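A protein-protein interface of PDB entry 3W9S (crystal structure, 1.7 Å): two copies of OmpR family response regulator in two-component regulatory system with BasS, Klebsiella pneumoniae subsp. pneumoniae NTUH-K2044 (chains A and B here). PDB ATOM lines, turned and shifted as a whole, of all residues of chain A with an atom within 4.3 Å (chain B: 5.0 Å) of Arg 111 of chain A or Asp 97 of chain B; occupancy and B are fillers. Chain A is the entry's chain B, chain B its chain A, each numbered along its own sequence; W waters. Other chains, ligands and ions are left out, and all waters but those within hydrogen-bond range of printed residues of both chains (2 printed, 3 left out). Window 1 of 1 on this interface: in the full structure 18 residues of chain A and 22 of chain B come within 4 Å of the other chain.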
ATOM      1  N   LEU A  76      13.107   2.998  -4.664  1.00  0.00           N
ATOM      2  CA  LEU A  76      12.574   1.771  -4.101  1.00  0.00           C
ATOM      3  C   LEU A  76      12.040   0.944  -5.264  1.00  0.00           C
ATOM      4  O   LEU A  76      11.160   1.391  -5.997  1.00  0.00           O
ATOM      5  CB  LEU A  76      11.460   2.074  -3.088  1.00  0.00           C
ATOM      6  CG  LEU A  76      10.896   0.872  -2.327  1.00  0.00           C
ATOM      7  CD1 LEU A  76      10.496   1.299  -0.918  1.00  0.00           C
ATOM      8  CD2 LEU A  76       9.688   0.311  -3.047  1.00  0.00           C
ATOM      9  N   ASP A  97      15.988   0.119  -1.710  1.00  0.00           N
ATOM     10  CA  ASP A  97      15.162  -0.916  -1.106  1.00  0.00           C
ATOM     11  C   ASP A  97      14.515  -1.673  -2.253  1.00  0.00           C
ATOM     12  O   ASP A  97      14.537  -1.221  -3.405  1.00  0.00           O
ATOM     13  CB  ASP A  97      14.113  -0.299  -0.169  1.00  0.00           C
ATOM     14  CG  ASP A  97      13.584  -1.281   0.872  1.00  0.00           C
ATOM     15  OD1 ASP A  97      13.784  -2.508   0.719  1.00  0.00           O
ATOM     16  OD2 ASP A  97      12.944  -0.816   1.839  1.00  0.00           O
ATOM     17  N   GLU A 107       3.138  -1.111   4.305  1.00  0.00           N
ATOM     18  CA  GLU A 107       4.582  -1.372   4.345  1.00  0.00           C
ATOM     19  C   GLU A 107       5.329  -0.512   3.336  1.00  0.00           C
ATOM     20  O   GLU A 107       6.419  -0.013   3.621  1.00  0.00           O
ATOM     21  CB  GLU A 107       4.921  -2.847   4.123  1.00  0.00           C
ATOM     22  CG  GLU A 107       6.435  -3.094   4.208  1.00  0.00           C
ATOM     23  CD  GLU A 107       6.809  -4.549   4.320  1.00  0.00           C
ATOM     24  OE1 GLU A 107       5.902  -5.414   4.327  1.00  0.00           O
ATOM     25  OE2 GLU A 107       8.033  -4.823   4.386  1.00  0.00           O
ATOM     26  N   LEU A 108       4.756  -0.345   2.146  1.00  0.00           N
ATOM     27  CA  LEU A 108       5.337   0.579   1.177  1.00  0.00           C
ATOM     28  C   LEU A 108       5.459   1.962   1.796  1.00  0.00           C
ATOM     29  O   LEU A 108       6.508   2.596   1.707  1.00  0.00           O
ATOM     30  CB  LEU A 108       4.488   0.643  -0.098  1.00  0.00           C
ATOM     31  CG  LEU A 108       4.956   1.694  -1.105  1.00  0.00           C
ATOM     32  CD1 LEU A 108       6.382   1.402  -1.582  1.00  0.00           C
ATOM     33  CD2 LEU A 108       4.005   1.782  -2.298  1.00  0.00           C
ATOM     34  N   ASN A 109       4.391   2.422   2.445  1.00  0.00           N
ATOM     35  CA  ASN A 109       4.418   3.735   3.073  1.00  0.00           C
ATOM     36  C   ASN A 109       5.517   3.848   4.123  1.00  0.00           C
ATOM     37  O   ASN A 109       6.219   4.859   4.192  1.00  0.00           O
ATOM     38  CB  ASN A 109       3.057   4.072   3.681  1.00  0.00           C
ATOM     39  CG  ASN A 109       2.001   4.312   2.625  1.00  0.00           C
ATOM     40  OD1 ASN A 109       2.324   4.613   1.473  1.00  0.00           O
ATOM     41  ND2 ASN A 109       0.730   4.189   3.009  1.00  0.00           N
ATOM     42  N   ALA A 110       5.673   2.807   4.931  1.00  0.00           N
ATOM     43  CA  ALA A 110       6.663   2.846   6.007  1.00  0.00           C
ATOM     44  C   ALA A 110       8.075   2.831   5.448  1.00  0.00           C
ATOM     45  O   ALA A 110       8.967   3.494   5.976  1.00  0.00           O
ATOM     46  CB  ALA A 110       6.463   1.683   6.966  1.00  0.00           C
ATOM     47  N   ARG A 111       8.279   2.069   4.377  1.00  0.00           N
ATOM     48  CA  ARG A 111       9.592   2.012   3.742  1.00  0.00           C
ATOM     49  C   ARG A 111       9.954   3.319   3.041  1.00  0.00           C
ATOM     50  O   ARG A 111      11.111   3.731   3.040  1.00  0.00           O
ATOM     51  CB  ARG A 111       9.694   0.799   2.810  1.00  0.00           C
ATOM     52  CG  ARG A 111       9.691  -0.506   3.609  1.00  0.00           C
ATOM     53  CD  ARG A 111       9.887  -1.752   2.749  1.00  0.00           C
ATOM     54  NE  ARG A 111       9.988  -2.929   3.606  1.00  0.00           N
ATOM     55  CZ  ARG A 111      11.131  -3.383   4.114  1.00  0.00           C
ATOM     56  NH1 ARG A 111      11.121  -4.457   4.896  1.00  0.00           N
ATOM     57  NH2 ARG A 111      12.277  -2.777   3.825  1.00  0.00           N
ATOM     58  N   ILE A 112       8.961   3.970   2.456  1.00  0.00           N
ATOM     59  CA  ILE A 112       9.179   5.284   1.878  1.00  0.00           C
ATOM     60  C   ILE A 112       9.519   6.299   2.975  1.00  0.00           C
ATOM     61  O   ILE A 112      10.438   7.097   2.817  1.00  0.00           O
ATOM     62  CB  ILE A 112       7.969   5.722   1.028  1.00  0.00           C
ATOM     63  CG1 ILE A 112       7.942   4.906  -0.262  1.00  0.00           C
ATOM     64  CG2 ILE A 112       8.032   7.214   0.720  1.00  0.00           C
ATOM     65  CD1 ILE A 112       6.688   5.122  -1.101  1.00  0.00           C
ATOM     66  N   ARG A 113       8.811   6.244   4.104  1.00  0.00           N
ATOM     67  CA  ARG A 113       9.158   7.117   5.231  1.00  0.00           C
ATOM     68  C   ARG A 113      10.598   6.892   5.685  1.00  0.00           C
ATOM     69  O   ARG A 113      11.322   7.848   5.935  1.00  0.00           O
ATOM     70  CB  ARG A 113       8.209   6.912   6.414  1.00  0.00           C
ATOM     71  CG  ARG A 113       6.827   7.483   6.194  1.00  0.00           C
ATOM     72  CD  ARG A 113       6.021   7.514   7.500  1.00  0.00           C
ATOM     73  NE  ARG A 113       5.719   6.191   8.049  1.00  0.00           N
ATOM     74  CZ  ARG A 113       4.667   5.450   7.710  1.00  0.00           C
ATOM     75  NH1 ARG A 113       4.471   4.273   8.285  1.00  0.00           N
ATOM     76  NH2 ARG A 113       3.808   5.875   6.790  1.00  0.00           N
ATOM     77  N   ALA A 114      11.007   5.627   5.787  1.00  0.00           N
ATOM     78  CA  ALA A 114      12.364   5.292   6.209  1.00  0.00           C
ATOM     79  C   ALA A 114      13.397   5.852   5.237  1.00  0.00           C
ATOM     80  O   ALA A 114      14.417   6.416   5.647  1.00  0.00           O
ATOM     81  CB  ALA A 114      12.526   3.767   6.345  1.00  0.00           C
ATOM     82  N   LEU A 115      13.132   5.700   3.945  1.00  0.00           N
ATOM     83  CA  LEU A 115      14.072   6.169   2.928  1.00  0.00           C
ATOM     84  C   LEU A 115      14.217   7.675   2.974  1.00  0.00           C
ATOM     85  O   LEU A 115      15.310   8.206   2.773  1.00  0.00           O
ATOM     86  CB  LEU A 115      13.617   5.742   1.531  1.00  0.00           C
ATOM     87  CG  LEU A 115      13.843   4.286   1.160  1.00  0.00           C
ATOM     88  CD1 LEU A 115      13.269   4.011  -0.234  1.00  0.00           C
ATOM     89  CD2 LEU A 115      15.323   3.981   1.195  1.00  0.00           C
ATOM     90  N   VAL B  75      20.466   1.304  10.920  1.00  0.00           N
ATOM     91  CA  VAL B  75      20.122   0.100  11.658  1.00  0.00           C
ATOM     92  C   VAL B  75      19.310  -0.813  10.761  1.00  0.00           C
ATOM     93  O   VAL B  75      18.293  -0.406  10.206  1.00  0.00           O
ATOM     94  CB  VAL B  75      19.278   0.424  12.907  1.00  0.00           C
ATOM     95  CG1 VAL B  75      18.715  -0.874  13.540  1.00  0.00           C
ATOM     96  CG2 VAL B  75      20.115   1.210  13.920  1.00  0.00           C
ATOM     97  N   LEU B  76      19.758  -2.055  10.623  1.00  0.00           N
ATOM     98  CA  LEU B  76      18.981  -3.053   9.903  1.00  0.00           C
ATOM     99  C   LEU B  76      18.447  -4.045  10.933  1.00  0.00           C
ATOM    100  O   LEU B  76      19.223  -4.680  11.650  1.00  0.00           O
ATOM    101  CB  LEU B  76      19.854  -3.757   8.854  1.00  0.00           C
ATOM    102  CG  LEU B  76      19.128  -4.753   7.940  1.00  0.00           C
ATOM    103  CD1 LEU B  76      19.778  -4.758   6.560  1.00  0.00           C
ATOM    104  CD2 LEU B  76      19.172  -6.154   8.533  1.00  0.00           C
ATOM    105  N   ILE B  77      17.127  -4.151  11.039  1.00  0.00           N
ATOM    106  CA  ILE B  77      16.519  -5.123  11.939  1.00  0.00           C
ATOM    107  C   ILE B  77      16.493  -6.479  11.240  1.00  0.00           C
ATOM    108  O   ILE B  77      16.108  -6.580  10.076  1.00  0.00           O
ATOM    109  CB  ILE B  77      15.091  -4.698  12.336  1.00  0.00           C
ATOM    110  CG1 ILE B  77      15.142  -3.586  13.386  1.00  0.00           C
ATOM    111  CG2 ILE B  77      14.311  -5.864  12.904  1.00  0.00           C
ATOM    112  CD1 ILE B  77      13.757  -3.018  13.704  1.00  0.00           C
ATOM    113  N   LEU B  91      10.262  -0.218  11.335  1.00  0.00           N
ATOM    114  CA  LEU B  91      10.668   0.896  10.495  1.00  0.00           C
ATOM    115  C   LEU B  91      10.317   2.240  11.151  1.00  0.00           C
ATOM    116  O   LEU B  91      11.157   3.140  11.233  1.00  0.00           O
ATOM    117  CB  LEU B  91      10.013   0.760   9.114  1.00  0.00           C
ATOM    118  CG  LEU B  91      10.512  -0.463   8.334  1.00  0.00           C
ATOM    119  CD1 LEU B  91       9.600  -0.781   7.157  1.00  0.00           C
ATOM    120  CD2 LEU B  91      11.945  -0.264   7.835  1.00  0.00           C
ATOM    121  N   ALA B  95      14.243   2.049  12.328  1.00  0.00           N
ATOM    122  CA  ALA B  95      15.102   1.152  11.557  1.00  0.00           C
ATOM    123  C   ALA B  95      15.114   1.588  10.096  1.00  0.00           C
ATOM    124  O   ALA B  95      14.110   2.090   9.585  1.00  0.00           O
ATOM    125  CB  ALA B  95      14.635  -0.286  11.674  1.00  0.00           C
ATOM    126  N   ASP B  96      16.246   1.389   9.429  1.00  0.00           N
ATOM    127  CA  ASP B  96      16.378   1.779   8.030  1.00  0.00           C
ATOM    128  C   ASP B  96      15.974   0.651   7.085  1.00  0.00           C
ATOM    129  O   ASP B  96      15.628   0.888   5.928  1.00  0.00           O
ATOM    130  CB  ASP B  96      17.812   2.226   7.774  1.00  0.00           C
ATOM    131  CG  ASP B  96      18.168   3.433   8.588  1.00  0.00           C
ATOM    132  OD1 ASP B  96      17.790   4.548   8.170  1.00  0.00           O
ATOM    133  OD2 ASP B  96      18.776   3.272   9.667  1.00  0.00           O
ATOM    134  N   ASP B  97      16.023  -0.578   7.583  1.00  0.00           N
ATOM    135  CA  ASP B  97      15.563  -1.734   6.824  1.00  0.00           C
ATOM    136  C   ASP B  97      15.151  -2.791   7.836  1.00  0.00           C
ATOM    137  O   ASP B  97      15.457  -2.683   9.027  1.00  0.00           O
ATOM    138  CB  ASP B  97      16.677  -2.255   5.897  1.00  0.00           C
ATOM    139  CG  ASP B  97      16.148  -3.057   4.711  1.00  0.00           C
ATOM    140  OD1 ASP B  97      14.972  -3.480   4.726  1.00  0.00           O
ATOM    141  OD2 ASP B  97      16.932  -3.284   3.763  1.00  0.00           O
ATOM    142  N   TYR B  98      14.430  -3.795   7.364  1.00  0.00           N
ATOM    143  CA  TYR B  98      13.848  -4.797   8.238  1.00  0.00           C
ATOM    144  C   TYR B  98      13.817  -6.069   7.422  1.00  0.00           C
ATOM    145  O   TYR B  98      13.117  -6.142   6.410  1.00  0.00           O
ATOM    146  CB  TYR B  98      12.431  -4.356   8.611  1.00  0.00           C
ATOM    147  CG  TYR B  98      11.768  -5.116   9.743  1.00  0.00           C
ATOM    148  CD1 TYR B  98      11.366  -6.434   9.586  1.00  0.00           C
ATOM    149  CD2 TYR B  98      11.504  -4.494  10.959  1.00  0.00           C
ATOM    150  CE1 TYR B  98      10.729  -7.118  10.622  1.00  0.00           C
ATOM    151  CE2 TYR B  98      10.876  -5.172  12.001  1.00  0.00           C
ATOM    152  CZ  TYR B  98      10.495  -6.483  11.826  1.00  0.00           C
ATOM    153  OH  TYR B  98       9.866  -7.165  12.856  1.00  0.00           O
ATOM    154  N   LEU B  99      14.605  -7.058   7.834  1.00  0.00           N
ATOM    155  CA  LEU B  99      14.732  -8.296   7.074  1.00  0.00           C
ATOM    156  C   LEU B  99      14.334  -9.465   7.965  1.00  0.00           C
ATOM    157  O   LEU B  99      14.884  -9.654   9.045  1.00  0.00           O
ATOM    158  CB  LEU B  99      16.173  -8.473   6.587  1.00  0.00           C
ATOM    159  CG  LEU B  99      16.523  -9.711   5.759  1.00  0.00           C
ATOM    160  CD1 LEU B  99      15.652  -9.780   4.507  1.00  0.00           C
ATOM    161  CD2 LEU B  99      18.007  -9.675   5.380  1.00  0.00           C
ATOM    162  N   ARG B 111      21.862  -5.730   1.270  1.00  0.00           N
ATOM    163  CA  ARG B 111      21.125  -4.682   1.971  1.00  0.00           C
ATOM    164  C   ARG B 111      22.047  -3.819   2.833  1.00  0.00           C
ATOM    165  O   ARG B 111      21.841  -2.607   2.960  1.00  0.00           O
ATOM    166  CB  ARG B 111      19.961  -5.276   2.775  1.00  0.00           C
ATOM    167  CG  ARG B 111      18.885  -5.841   1.843  1.00  0.00           C
ATOM    168  CD  ARG B 111      17.635  -6.330   2.577  1.00  0.00           C
ATOM    169  NE  ARG B 111      16.606  -6.701   1.609  1.00  0.00           N
ATOM    170  CZ  ARG B 111      15.710  -5.852   1.111  1.00  0.00           C
ATOM    171  NH1 ARG B 111      14.822  -6.283   0.224  1.00  0.00           N
ATOM    172  NH2 ARG B 111      15.693  -4.580   1.505  1.00  0.00           N
ATOM    173  N   LEU B 115      22.644   0.204   2.406  1.00  0.00           N
ATOM    174  CA  LEU B 115      22.547   1.152   3.519  1.00  0.00           C
ATOM    175  C   LEU B 115      23.796   2.004   3.640  1.00  0.00           C
ATOM    176  O   LEU B 115      23.718   3.194   3.948  1.00  0.00           O
ATOM    177  CB  LEU B 115      22.301   0.424   4.843  1.00  0.00           C
ATOM    178  CG  LEU B 115      20.906  -0.147   5.056  1.00  0.00           C
ATOM    179  CD1 LEU B 115      20.849  -0.892   6.389  1.00  0.00           C
ATOM    180  CD2 LEU B 115      19.887   0.969   5.039  1.00  0.00           C
HETATM  181  O   HOH W   1      16.819   5.040   5.685  1.00  0.00           O
HETATM  182  O   HOH W   2       9.277   4.204   8.692  1.00  0.00           O
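OD1 of Asp 97 of chain A is in salt-bridge range of NH2 of Arg 111 of chain B (2.9 Å).
NH2 of Arg 111 of chain A is in salt-bridge range of OD1 of Asp 97 of chain B (2.9 Å).
The backbone carbonyl oxygen of Tyr 98 of chain B sits at hydrogen-bond distance from the guanidinium group of Arg 111 of chain A (3.0 Å).
Asp 97 of chain A touches Arg 111 of chain B, and with the chains exchanged Arg 111 of chain A touches Asp 97 of chain B.
Positions printed for both chains: 76, 97, 111 and 115.
The side-chain carboxylate of Asp 97 of chain A lies within salt-bridge range of the guanidinium group of Arg 111 of chain A (2.9 Å).
OE2 of Glu 107 of chain A is in salt-bridge range of NE of Arg 111 of chain A, 2.8 Å away.
N of Ile 77 of chain B sits at hydrogen-bond distance from O of Asp 97 of chain B (3.0 Å).
The backbone carbonyl oxygen (O) of Val 75 of chain B is in hydrogen-bond range of the backbone NH (N) of Asp 97 of chain B (3.5 Å).
The side-chain carboxylate of Asp 97 of chain B is in salt-bridge range of the guanidinium group of Arg 111 of chain B (2.9 Å).
Of the 11 printed residues of chain B, 5 touch a printed residue of chain A.
Hydrophobic or aromatic side chains of chain B within 4 Å of the printed part of chain A: Leu 91 and Tyr 98.
Among the printed residues, 6 pairs touch across the chains.
Among the printed residues, Asp or Glu carboxylates within 4 Å of a Lys or Arg side-chain nitrogen of the other chain: Asp 97 of chain A with Arg 111 of chain B (2.9 Å) and Arg 111 of chain A with Asp 97 of chain B (2.9 Å).
Water W1 bridges the side-chain carboxylate (OD1) of Asp 96 of chain B and the backbone carbonyl oxygen (O) of Ala 114 of chain A.
Water W2 lies within hydrogen-bond range of the backbone carbonyl oxygen of Ala 110 of chain A (2.8 Å) and the backbone carbonyl oxygen of Leu 91 of chain B (3.3 Å).
Among the printed residues, pairs that only touch across the chains: Ala 110 of chain A with Leu 91 of chain B (3.99 Å), Arg 111 of chain A with Leu 91 of chain B (3.6 Å) and Ala 114 of chain A with Ala 95 of chain B (3.98 Å).
Of chain B, only Leu 91, Asp 97 and Tyr 98 come within 4 Å of Arg 111 of chain A.
Of the printed residues of chain A, Ala 95 of chain B touches Ala 114 (3.98 Å).
Asp 97 of chain B touches just one residue of chain A: Arg 111 (2.9 Å).
Leu 99 of chain B touches none of the printed residues of chain A.
Printed residues of chain A within 4 Å of Arg 111 of chain B: Asp 97 (2.9 Å).
The nearest residue of chain B that does not touch Arg 111 of chain A is Arg 111 of chain B (4.5 Å).
The nearest printed residue of chain A that does not touch Asp 97 of chain B is Asp 97 of chain A (4.3 Å).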
